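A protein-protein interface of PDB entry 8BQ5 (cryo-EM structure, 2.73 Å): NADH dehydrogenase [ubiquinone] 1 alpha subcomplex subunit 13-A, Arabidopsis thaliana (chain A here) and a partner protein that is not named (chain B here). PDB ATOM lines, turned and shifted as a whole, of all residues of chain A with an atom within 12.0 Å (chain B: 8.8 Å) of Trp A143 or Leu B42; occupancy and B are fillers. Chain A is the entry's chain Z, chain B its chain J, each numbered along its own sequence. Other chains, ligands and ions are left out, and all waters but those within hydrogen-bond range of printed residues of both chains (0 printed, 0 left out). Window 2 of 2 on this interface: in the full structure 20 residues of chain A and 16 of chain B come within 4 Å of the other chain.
OG1 of Thr A135 sits at hydrogen-bond distance from N of Glu A137 (3.2 Å).
Among the printed residues, merely in contact across the chains: Leu A138 with Leu B44, Arg A139 with Gly B45 and Trp A143 with Leu B42.
Of the 23 printed residues of chain B, 5 touch a printed residue of chain A. Printed residues of chain B that touch a printed residue of chain A: Leu B42, Leu B43, Leu B44, Gly B45 and Arg B123. Of the 9 printed residues of chain A, 4 touch a printed residue of chain B. Hydrophobic or aromatic side chains of chain A within 4 Å of the printed part of chain B: Leu A138 and Trp A143. Among the printed residues, 6 pairs touch across the chains.
Of the printed residues of chain B, Leu A138 touches Leu B44 (3.5 Å). Trp A143 touches two residues of chain B. No residue of chain A comes within 4 Å of Ser B38. No residue of chain A comes within 4 Å of Gly B39. Of chain A, only Trp A143 (3.5 Å) comes within 4 Å of Leu B43. Of chain A, only Leu A138 (3.5 Å) and Arg A139 (3.2 Å) come within 4 Å of Leu B44. No residue of chain A comes within 4 Å of Asp B47. No residue of chain A comes within 4 Å of Ala B50. Of the printed residues of chain A, Arg B123 touches Glu A137 (2.9 Å). Asn B136 touches none of the printed residues of chain A. The nearest printed residue of chain B that does not touch Arg A139 is Leu B46 (4.001 Å).
The guanidinium group (NH2) of Arg B123 is in salt-bridge range of the side-chain carboxylate (OE2) of Glu A137 (2.9 Å). O of Leu B43 is in hydrogen-bond range of NE1 of Trp A143. The backbone carbonyl oxygen of Leu B44 lies close to the guanidinium group of Arg A139, 3.2 Å away.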
ATOM      1  N   THR A 135      -7.036  20.880 -26.683  1.00  0.00           N
ATOM      2  CA  THR A 135      -7.419  22.259 -26.267  1.00  0.00           C
ATOM      3  C   THR A 135      -6.237  23.222 -26.163  1.00  0.00           C
ATOM      4  O   THR A 135      -6.490  24.437 -26.235  1.00  0.00           O
ATOM      5  CB  THR A 135      -8.183  22.236 -24.934  1.00  0.00           C
ATOM      6  OG1 THR A 135      -7.265  21.990 -23.867  1.00  0.00           O
ATOM      7  CG2 THR A 135      -9.276  21.191 -24.900  1.00  0.00           C
ATOM      8  N   GLY A 136      -5.015  22.739 -25.967  1.00  0.00           N
ATOM      9  CA  GLY A 136      -3.920  23.664 -25.768  1.00  0.00           C
ATOM     10  C   GLY A 136      -3.779  24.172 -24.353  1.00  0.00           C
ATOM     11  O   GLY A 136      -2.940  25.041 -24.097  1.00  0.00           O
ATOM     12  N   GLU A 137      -4.605  23.644 -23.450  1.00  0.00           N
ATOM     13  CA  GLU A 137      -4.550  23.992 -22.011  1.00  0.00           C
ATOM     14  C   GLU A 137      -3.988  22.768 -21.285  1.00  0.00           C
ATOM     15  O   GLU A 137      -4.378  21.642 -21.644  1.00  0.00           O
ATOM     16  CB  GLU A 137      -5.947  24.379 -21.541  1.00  0.00           C
ATOM     17  CG  GLU A 137      -6.349  25.781 -21.947  1.00  0.00           C
ATOM     18  CD  GLU A 137      -7.746  25.884 -22.532  1.00  0.00           C
ATOM     19  OE1 GLU A 137      -7.935  25.458 -23.687  1.00  0.00           O
ATOM     20  OE2 GLU A 137      -8.643  26.390 -21.830  1.00  0.00           O
ATOM     21  N   LEU A 138      -3.101  22.971 -20.311  1.00  0.00           N
ATOM     22  CA  LEU A 138      -2.431  21.837 -19.684  1.00  0.00           C
ATOM     23  C   LEU A 138      -3.379  21.059 -18.780  1.00  0.00           C
ATOM     24  O   LEU A 138      -3.493  19.832 -18.890  1.00  0.00           O
ATOM     25  CB  LEU A 138      -1.211  22.327 -18.904  1.00  0.00           C
ATOM     26  CG  LEU A 138       0.152  22.034 -19.535  1.00  0.00           C
ATOM     27  CD1 LEU A 138       1.239  22.022 -18.481  1.00  0.00           C
ATOM     28  CD2 LEU A 138       0.133  20.718 -20.294  1.00  0.00           C
ATOM     29  N   ARG A 139      -4.073  21.752 -17.882  1.00  0.00           N
ATOM     30  CA  ARG A 139      -4.956  21.120 -16.901  1.00  0.00           C
ATOM     31  C   ARG A 139      -6.269  21.889 -16.832  1.00  0.00           C
ATOM     32  O   ARG A 139      -6.558  22.564 -15.836  1.00  0.00           O
ATOM     33  CB  ARG A 139      -4.281  21.058 -15.532  1.00  0.00           C
ATOM     34  CG  ARG A 139      -4.800  19.961 -14.625  1.00  0.00           C
ATOM     35  CD  ARG A 139      -4.179  18.622 -14.968  1.00  0.00           C
ATOM     36  NE  ARG A 139      -4.933  17.515 -14.395  1.00  0.00           N
ATOM     37  CZ  ARG A 139      -4.736  17.032 -13.176  1.00  0.00           C
ATOM     38  NH1 ARG A 139      -3.814  17.538 -12.373  1.00  0.00           N
ATOM     39  NH2 ARG A 139      -5.484  16.018 -12.752  1.00  0.00           N
ATOM     40  N   PRO A 140      -7.173  21.861 -17.858  1.00  0.00           N
ATOM     41  CA  PRO A 140      -8.405  22.643 -17.769  1.00  0.00           C
ATOM     42  C   PRO A 140      -9.474  21.931 -16.932  1.00  0.00           C
ATOM     43  O   PRO A 140     -10.390  22.587 -16.509  1.00  0.00           O
ATOM     44  CB  PRO A 140      -8.874  22.740 -19.231  1.00  0.00           C
ATOM     45  CG  PRO A 140      -8.436  21.450 -19.861  1.00  0.00           C
ATOM     46  CD  PRO A 140      -7.140  21.117 -19.158  1.00  0.00           C
ATOM     47  N   ASP A 141      -9.314  20.626 -16.692  1.00  0.00           N
ATOM     48  CA  ASP A 141     -10.358  19.840 -15.983  1.00  0.00           C
ATOM     49  C   ASP A 141     -10.344  20.096 -14.470  1.00  0.00           C
ATOM     50  O   ASP A 141     -11.275  19.616 -13.811  1.00  0.00           O
ATOM     51  CB  ASP A 141     -10.225  18.345 -16.289  1.00  0.00           C
ATOM     52  CG  ASP A 141     -10.647  17.982 -17.705  1.00  0.00           C
ATOM     53  OD1 ASP A 141     -11.238  16.894 -17.882  1.00  0.00           O
ATOM     54  OD2 ASP A 141     -10.375  18.781 -18.621  1.00  0.00           O
ATOM     55  N   VAL A 142      -9.332  20.788 -13.938  1.00  0.00           N
ATOM     56  CA  VAL A 142      -9.234  20.983 -12.457  1.00  0.00           C
ATOM     57  C   VAL A 142      -9.787  22.361 -12.079  1.00  0.00           C
ATOM     58  O   VAL A 142      -9.923  22.632 -10.877  1.00  0.00           O
ATOM     59  CB  VAL A 142      -7.802  20.787 -11.928  1.00  0.00           C
ATOM     60  CG1 VAL A 142      -7.291  19.382 -12.192  1.00  0.00           C
ATOM     61  CG2 VAL A 142      -6.834  21.839 -12.440  1.00  0.00           C
ATOM     62  N   TRP A 143     -10.106  23.183 -13.074  1.00  0.00           N
ATOM     63  CA  TRP A 143     -10.648  24.535 -12.801  1.00  0.00           C
ATOM     64  C   TRP A 143     -12.058  24.649 -13.395  1.00  0.00           C
ATOM     65  O   TRP A 143     -12.743  25.626 -13.044  1.00  0.00           O
ATOM     66  CB  TRP A 143      -9.689  25.596 -13.347  1.00  0.00           C
ATOM     67  CG  TRP A 143      -8.396  25.701 -12.597  1.00  0.00           C
ATOM     68  CD1 TRP A 143      -7.167  25.286 -13.020  1.00  0.00           C
ATOM     69  CD2 TRP A 143      -8.193  26.274 -11.292  1.00  0.00           C
ATOM     70  NE1 TRP A 143      -6.219  25.552 -12.072  1.00  0.00           N
ATOM     71  CE2 TRP A 143      -6.817  26.160 -11.002  1.00  0.00           C
ATOM     72  CE3 TRP A 143      -9.034  26.870 -10.346  1.00  0.00           C
ATOM     73  CZ2 TRP A 143      -6.269  26.623  -9.808  1.00  0.00           C
ATOM     74  CZ3 TRP A 143      -8.491  27.327  -9.166  1.00  0.00           C
ATOM     75  CH2 TRP A 143      -7.127  27.203  -8.901  1.00  0.00           C
ATOM     76  N   ILE B   2      -1.536  35.121 -15.550  1.00  0.00           N
ATOM     77  CA  ILE B   2      -1.135  34.672 -14.219  1.00  0.00           C
ATOM     78  C   ILE B   2       0.220  33.980 -14.283  1.00  0.00           C
ATOM     79  O   ILE B   2       1.070  34.156 -13.399  1.00  0.00           O
ATOM     80  CB  ILE B   2      -2.215  33.757 -13.611  1.00  0.00           C
ATOM     81  CG1 ILE B   2      -3.486  34.557 -13.325  1.00  0.00           C
ATOM     82  CG2 ILE B   2      -1.699  33.087 -12.342  1.00  0.00           C
ATOM     83  CD1 ILE B   2      -4.385  33.933 -12.276  1.00  0.00           C
ATOM     84  N   LEU B   6       3.551  35.033 -12.110  1.00  0.00           N
ATOM     85  CA  LEU B   6       4.385  34.106 -11.349  1.00  0.00           C
ATOM     86  C   LEU B   6       5.784  34.016 -11.946  1.00  0.00           C
ATOM     87  O   LEU B   6       6.776  33.965 -11.213  1.00  0.00           O
ATOM     88  CB  LEU B   6       3.730  32.726 -11.281  1.00  0.00           C
ATOM     89  CG  LEU B   6       2.469  32.563 -10.424  1.00  0.00           C
ATOM     90  CD1 LEU B   6       2.150  31.094 -10.216  1.00  0.00           C
ATOM     91  CD2 LEU B   6       2.607  33.261  -9.080  1.00  0.00           C
ATOM     92  N   CYS B  35       7.866  29.327  -2.782  1.00  0.00           N
ATOM     93  CA  CYS B  35       6.440  29.640  -2.688  1.00  0.00           C
ATOM     94  C   CYS B  35       5.839  29.869  -4.070  1.00  0.00           C
ATOM     95  O   CYS B  35       4.732  29.399  -4.379  1.00  0.00           O
ATOM     96  CB  CYS B  35       6.229  30.872  -1.805  1.00  0.00           C
ATOM     97  SG  CYS B  35       6.589  30.627  -0.057  1.00  0.00           S
ATOM     98  N   ASP B  36       6.563  30.596  -4.918  1.00  0.00           N
ATOM     99  CA  ASP B  36       6.097  30.839  -6.279  1.00  0.00           C
ATOM    100  C   ASP B  36       5.949  29.535  -7.060  1.00  0.00           C
ATOM    101  O   ASP B  36       4.963  29.330  -7.788  1.00  0.00           O
ATOM    102  CB  ASP B  36       7.079  31.774  -6.969  1.00  0.00           C
ATOM    103  CG  ASP B  36       6.403  32.755  -7.857  1.00  0.00           C
ATOM    104  OD1 ASP B  36       6.855  32.875  -9.001  1.00  0.00           O
ATOM    105  OD2 ASP B  36       5.434  33.408  -7.415  1.00  0.00           O
ATOM    106  N   THR B  37       6.928  28.642  -6.915  1.00  0.00           N
ATOM    107  CA  THR B  37       6.861  27.331  -7.549  1.00  0.00           C
ATOM    108  C   THR B  37       5.636  26.554  -7.077  1.00  0.00           C
ATOM    109  O   THR B  37       4.966  25.881  -7.873  1.00  0.00           O
ATOM    110  CB  THR B  37       8.142  26.558  -7.239  1.00  0.00           C
ATOM    111  OG1 THR B  37       9.226  27.097  -8.004  1.00  0.00           O
ATOM    112  CG2 THR B  37       7.977  25.093  -7.555  1.00  0.00           C
ATOM    113  N   SER B  38       5.338  26.632  -5.780  1.00  0.00           N
ATOM    114  CA  SER B  38       4.151  25.975  -5.243  1.00  0.00           C
ATOM    115  C   SER B  38       2.877  26.520  -5.878  1.00  0.00           C
ATOM    116  O   SER B  38       1.937  25.763  -6.153  1.00  0.00           O
ATOM    117  CB  SER B  38       4.111  26.148  -3.725  1.00  0.00           C
ATOM    118  OG  SER B  38       2.976  25.518  -3.165  1.00  0.00           O
ATOM    119  N   GLY B  39       2.818  27.834  -6.096  1.00  0.00           N
ATOM    120  CA  GLY B  39       1.664  28.395  -6.790  1.00  0.00           C
ATOM    121  C   GLY B  39       1.522  27.848  -8.199  1.00  0.00           C
ATOM    122  O   GLY B  39       0.419  27.516  -8.657  1.00  0.00           O
ATOM    123  N   LEU B  40       2.649  27.725  -8.898  1.00  0.00           N
ATOM    124  CA  LEU B  40       2.632  27.147 -10.238  1.00  0.00           C
ATOM    125  C   LEU B  40       2.096  25.713 -10.204  1.00  0.00           C
ATOM    126  O   LEU B  40       1.277  25.311 -11.048  1.00  0.00           O
ATOM    127  CB  LEU B  40       4.050  27.165 -10.799  1.00  0.00           C
ATOM    128  CG  LEU B  40       4.257  26.526 -12.152  1.00  0.00           C
ATOM    129  CD1 LEU B  40       3.282  27.235 -12.986  1.00  0.00           C
ATOM    130  CD2 LEU B  40       5.651  26.765 -12.638  1.00  0.00           C
ATOM    131  N   LEU B  41       2.547  24.931  -9.220  1.00  0.00           N
ATOM    132  CA  LEU B  41       2.097  23.550  -9.081  1.00  0.00           C
ATOM    133  C   LEU B  41       0.602  23.482  -8.799  1.00  0.00           C
ATOM    134  O   LEU B  41      -0.091  22.582  -9.288  1.00  0.00           O
ATOM    135  CB  LEU B  41       2.883  22.859  -7.970  1.00  0.00           C
ATOM    136  CG  LEU B  41       4.326  22.509  -8.330  1.00  0.00           C
ATOM    137  CD1 LEU B  41       5.033  21.866  -7.153  1.00  0.00           C
ATOM    138  CD2 LEU B  41       4.361  21.601  -9.546  1.00  0.00           C
ATOM    139  N   LEU B  42       0.090  24.414  -7.993  1.00  0.00           N
ATOM    140  CA  LEU B  42      -1.351  24.467  -7.761  1.00  0.00           C
ATOM    141  C   LEU B  42      -2.100  24.737  -9.057  1.00  0.00           C
ATOM    142  O   LEU B  42      -3.185  24.190  -9.284  1.00  0.00           O
ATOM    143  CB  LEU B  42      -1.686  25.533  -6.722  1.00  0.00           C
ATOM    144  CG  LEU B  42      -1.639  25.088  -5.264  1.00  0.00           C
ATOM    145  CD1 LEU B  42      -2.009  26.238  -4.354  1.00  0.00           C
ATOM    146  CD2 LEU B  42      -2.570  23.911  -5.043  1.00  0.00           C
ATOM    147  N   LEU B  43      -1.541  25.592  -9.914  1.00  0.00           N
ATOM    148  CA  LEU B  43      -2.150  25.796 -11.226  1.00  0.00           C
ATOM    149  C   LEU B  43      -2.141  24.522 -12.059  1.00  0.00           C
ATOM    150  O   LEU B  43      -3.052  24.301 -12.864  1.00  0.00           O
ATOM    151  CB  LEU B  43      -1.438  26.908 -11.981  1.00  0.00           C
ATOM    152  CG  LEU B  43      -2.075  28.276 -11.812  1.00  0.00           C
ATOM    153  CD1 LEU B  43      -1.262  29.257 -12.579  1.00  0.00           C
ATOM    154  CD2 LEU B  43      -3.487  28.255 -12.333  1.00  0.00           C
ATOM    155  N   LEU B  44      -1.117  23.687 -11.899  1.00  0.00           N
ATOM    156  CA  LEU B  44      -1.084  22.413 -12.611  1.00  0.00           C
ATOM    157  C   LEU B  44      -2.079  21.389 -12.075  1.00  0.00           C
ATOM    158  O   LEU B  44      -2.263  20.346 -12.709  1.00  0.00           O
ATOM    159  CB  LEU B  44       0.322  21.813 -12.566  1.00  0.00           C
ATOM    160  CG  LEU B  44       1.338  22.410 -13.534  1.00  0.00           C
ATOM    161  CD1 LEU B  44       2.731  21.902 -13.220  1.00  0.00           C
ATOM    162  CD2 LEU B  44       0.946  22.080 -14.954  1.00  0.00           C
ATOM    163  N   GLY B  45      -2.717  21.646 -10.936  1.00  0.00           N
ATOM    164  CA  GLY B  45      -3.625  20.682 -10.349  1.00  0.00           C
ATOM    165  C   GLY B  45      -2.982  19.654  -9.447  1.00  0.00           C
ATOM    166  O   GLY B  45      -3.669  18.729  -9.002  1.00  0.00           O
ATOM    167  N   LEU B  46      -1.688  19.789  -9.157  1.00  0.00           N
ATOM    168  CA  LEU B  46      -0.957  18.836  -8.322  1.00  0.00           C
ATOM    169  C   LEU B  46      -0.820  19.435  -6.925  1.00  0.00           C
ATOM    170  O   LEU B  46       0.194  20.037  -6.570  1.00  0.00           O
ATOM    171  CB  LEU B  46       0.398  18.518  -8.945  1.00  0.00           C
ATOM    172  CG  LEU B  46       0.390  18.253 -10.451  1.00  0.00           C
ATOM    173  CD1 LEU B  46       1.791  18.352 -11.024  1.00  0.00           C
ATOM    174  CD2 LEU B  46      -0.216  16.892 -10.747  1.00  0.00           C
ATOM    175  N   ASP B  47      -1.870  19.259  -6.118  1.00  0.00           N
ATOM    176  CA  ASP B  47      -1.901  19.888  -4.801  1.00  0.00           C
ATOM    177  C   ASP B  47      -0.932  19.224  -3.834  1.00  0.00           C
ATOM    178  O   ASP B  47      -0.333  19.906  -2.995  1.00  0.00           O
ATOM    179  CB  ASP B  47      -3.311  19.848  -4.217  1.00  0.00           C
ATOM    180  CG  ASP B  47      -4.032  18.556  -4.524  1.00  0.00           C
ATOM    181  OD1 ASP B  47      -5.273  18.572  -4.628  1.00  0.00           O
ATOM    182  OD2 ASP B  47      -3.357  17.516  -4.656  1.00  0.00           O
ATOM    183  N   PHE B  48      -0.783  17.899  -3.916  1.00  0.00           N
ATOM    184  CA  PHE B  48       0.144  17.203  -3.029  1.00  0.00           C
ATOM    185  C   PHE B  48       1.566  17.701  -3.228  1.00  0.00           C
ATOM    186  O   PHE B  48       2.281  17.964  -2.259  1.00  0.00           O
ATOM    187  CB  PHE B  48       0.072  15.696  -3.259  1.00  0.00           C
ATOM    188  CG  PHE B  48       1.179  14.930  -2.591  1.00  0.00           C
ATOM    189  CD1 PHE B  48       1.161  14.714  -1.224  1.00  0.00           C
ATOM    190  CD2 PHE B  48       2.237  14.426  -3.330  1.00  0.00           C
ATOM    191  CE1 PHE B  48       2.171  14.005  -0.607  1.00  0.00           C
ATOM    192  CE2 PHE B  48       3.254  13.722  -2.718  1.00  0.00           C
ATOM    193  CZ  PHE B  48       3.221  13.510  -1.352  1.00  0.00           C
ATOM    194  N   PHE B  49       1.991  17.842  -4.484  1.00  0.00           N
ATOM    195  CA  PHE B  49       3.336  18.339  -4.747  1.00  0.00           C
ATOM    196  C   PHE B  49       3.473  19.801  -4.342  1.00  0.00           C
ATOM    197  O   PHE B  49       4.523  20.213  -3.839  1.00  0.00           O
ATOM    198  CB  PHE B  49       3.687  18.140  -6.218  1.00  0.00           C
ATOM    199  CG  PHE B  49       4.175  16.759  -6.535  1.00  0.00           C
ATOM    200  CD1 PHE B  49       5.465  16.377  -6.209  1.00  0.00           C
ATOM    201  CD2 PHE B  49       3.341  15.838  -7.143  1.00  0.00           C
ATOM    202  CE1 PHE B  49       5.917  15.105  -6.494  1.00  0.00           C
ATOM    203  CE2 PHE B  49       3.787  14.563  -7.429  1.00  0.00           C
ATOM    204  CZ  PHE B  49       5.077  14.196  -7.105  1.00  0.00           C
ATOM    205  N   ALA B  50       2.418  20.594  -4.535  1.00  0.00           N
ATOM    206  CA  ALA B  50       2.459  21.991  -4.119  1.00  0.00           C
ATOM    207  C   ALA B  50       2.636  22.115  -2.610  1.00  0.00           C
ATOM    208  O   ALA B  50       3.366  22.990  -2.132  1.00  0.00           O
ATOM    209  CB  ALA B  50       1.192  22.713  -4.574  1.00  0.00           C
ATOM    210  N   MET B  51       1.971  21.248  -1.843  1.00  0.00           N
ATOM    211  CA  MET B  51       2.101  21.290  -0.390  1.00  0.00           C
ATOM    212  C   MET B  51       3.427  20.692   0.066  1.00  0.00           C
ATOM    213  O   MET B  51       4.026  21.157   1.043  1.00  0.00           O
ATOM    214  CB  MET B  51       0.931  20.551   0.260  1.00  0.00           C
ATOM    215  CG  MET B  51      -0.407  21.279   0.188  1.00  0.00           C
ATOM    216  SD  MET B  51      -0.416  22.936   0.900  1.00  0.00           S
ATOM    217  CE  MET B  51      -0.324  23.952  -0.573  1.00  0.00           C
ATOM    218  N   LEU B  54       6.264  23.054   0.014  1.00  0.00           N
ATOM    219  CA  LEU B  54       6.305  23.888   1.211  1.00  0.00           C
ATOM    220  C   LEU B  54       6.854  23.113   2.401  1.00  0.00           C
ATOM    221  O   LEU B  54       7.679  23.627   3.167  1.00  0.00           O
ATOM    222  CB  LEU B  54       4.909  24.424   1.523  1.00  0.00           C
ATOM    223  CG  LEU B  54       4.193  25.130   0.375  1.00  0.00           C
ATOM    224  CD1 LEU B  54       2.820  25.563   0.817  1.00  0.00           C
ATOM    225  CD2 LEU B  54       4.999  26.321  -0.111  1.00  0.00           C
ATOM    226  N   ARG B 123     -15.021  21.279 -26.466  1.00  0.00           N
ATOM    227  CA  ARG B 123     -14.542  20.443 -25.337  1.00  0.00           C
ATOM    228  C   ARG B 123     -15.482  19.247 -25.186  1.00  0.00           C
ATOM    229  O   ARG B 123     -16.627  19.451 -24.746  1.00  0.00           O
ATOM    230  CB  ARG B 123     -14.490  21.243 -24.032  1.00  0.00           C
ATOM    231  CG  ARG B 123     -13.446  22.348 -24.018  1.00  0.00           C
ATOM    232  CD  ARG B 123     -13.423  23.059 -22.680  1.00  0.00           C
ATOM    233  NE  ARG B 123     -12.485  24.172 -22.646  1.00  0.00           N
ATOM    234  CZ  ARG B 123     -12.361  25.019 -21.632  1.00  0.00           C
ATOM    235  NH1 ARG B 123     -13.121  24.884 -20.559  1.00  0.00           N
ATOM    236  NH2 ARG B 123     -11.478  26.001 -21.690  1.00  0.00           N
ATOM    237  N   LYS B 130     -15.252  10.389 -14.432  1.00  0.00           N
ATOM    238  CA  LYS B 130     -15.623  11.316 -13.375  1.00  0.00           C
ATOM    239  C   LYS B 130     -16.513  10.686 -12.314  1.00  0.00           C
ATOM    240  O   LYS B 130     -16.929  11.381 -11.384  1.00  0.00           O
ATOM    241  CB  LYS B 130     -16.332  12.533 -13.970  1.00  0.00           C
ATOM    242  CG  LYS B 130     -15.409  13.559 -14.583  1.00  0.00           C
ATOM    243  CD  LYS B 130     -16.205  14.590 -15.361  1.00  0.00           C
ATOM    244  CE  LYS B 130     -15.331  15.318 -16.363  1.00  0.00           C
ATOM    245  NZ  LYS B 130     -15.049  16.715 -15.937  1.00  0.00           N
ATOM    246  N   ASN B 136      -4.468  13.402  -6.600  1.00  0.00           N
ATOM    247  CA  ASN B 136      -3.071  13.227  -6.979  1.00  0.00           C
ATOM    248  C   ASN B 136      -2.336  12.407  -5.921  1.00  0.00           C
ATOM    249  O   ASN B 136      -1.449  11.599  -6.239  1.00  0.00           O
ATOM    250  CB  ASN B 136      -2.442  14.609  -7.200  1.00  0.00           C
ATOM    251  CG  ASN B 136      -0.930  14.603  -7.123  1.00  0.00           C
ATOM    252  OD1 ASN B 136      -0.267  13.768  -7.732  1.00  0.00           O
ATOM    253  ND2 ASN B 136      -0.377  15.578  -6.419  1.00  0.00           N
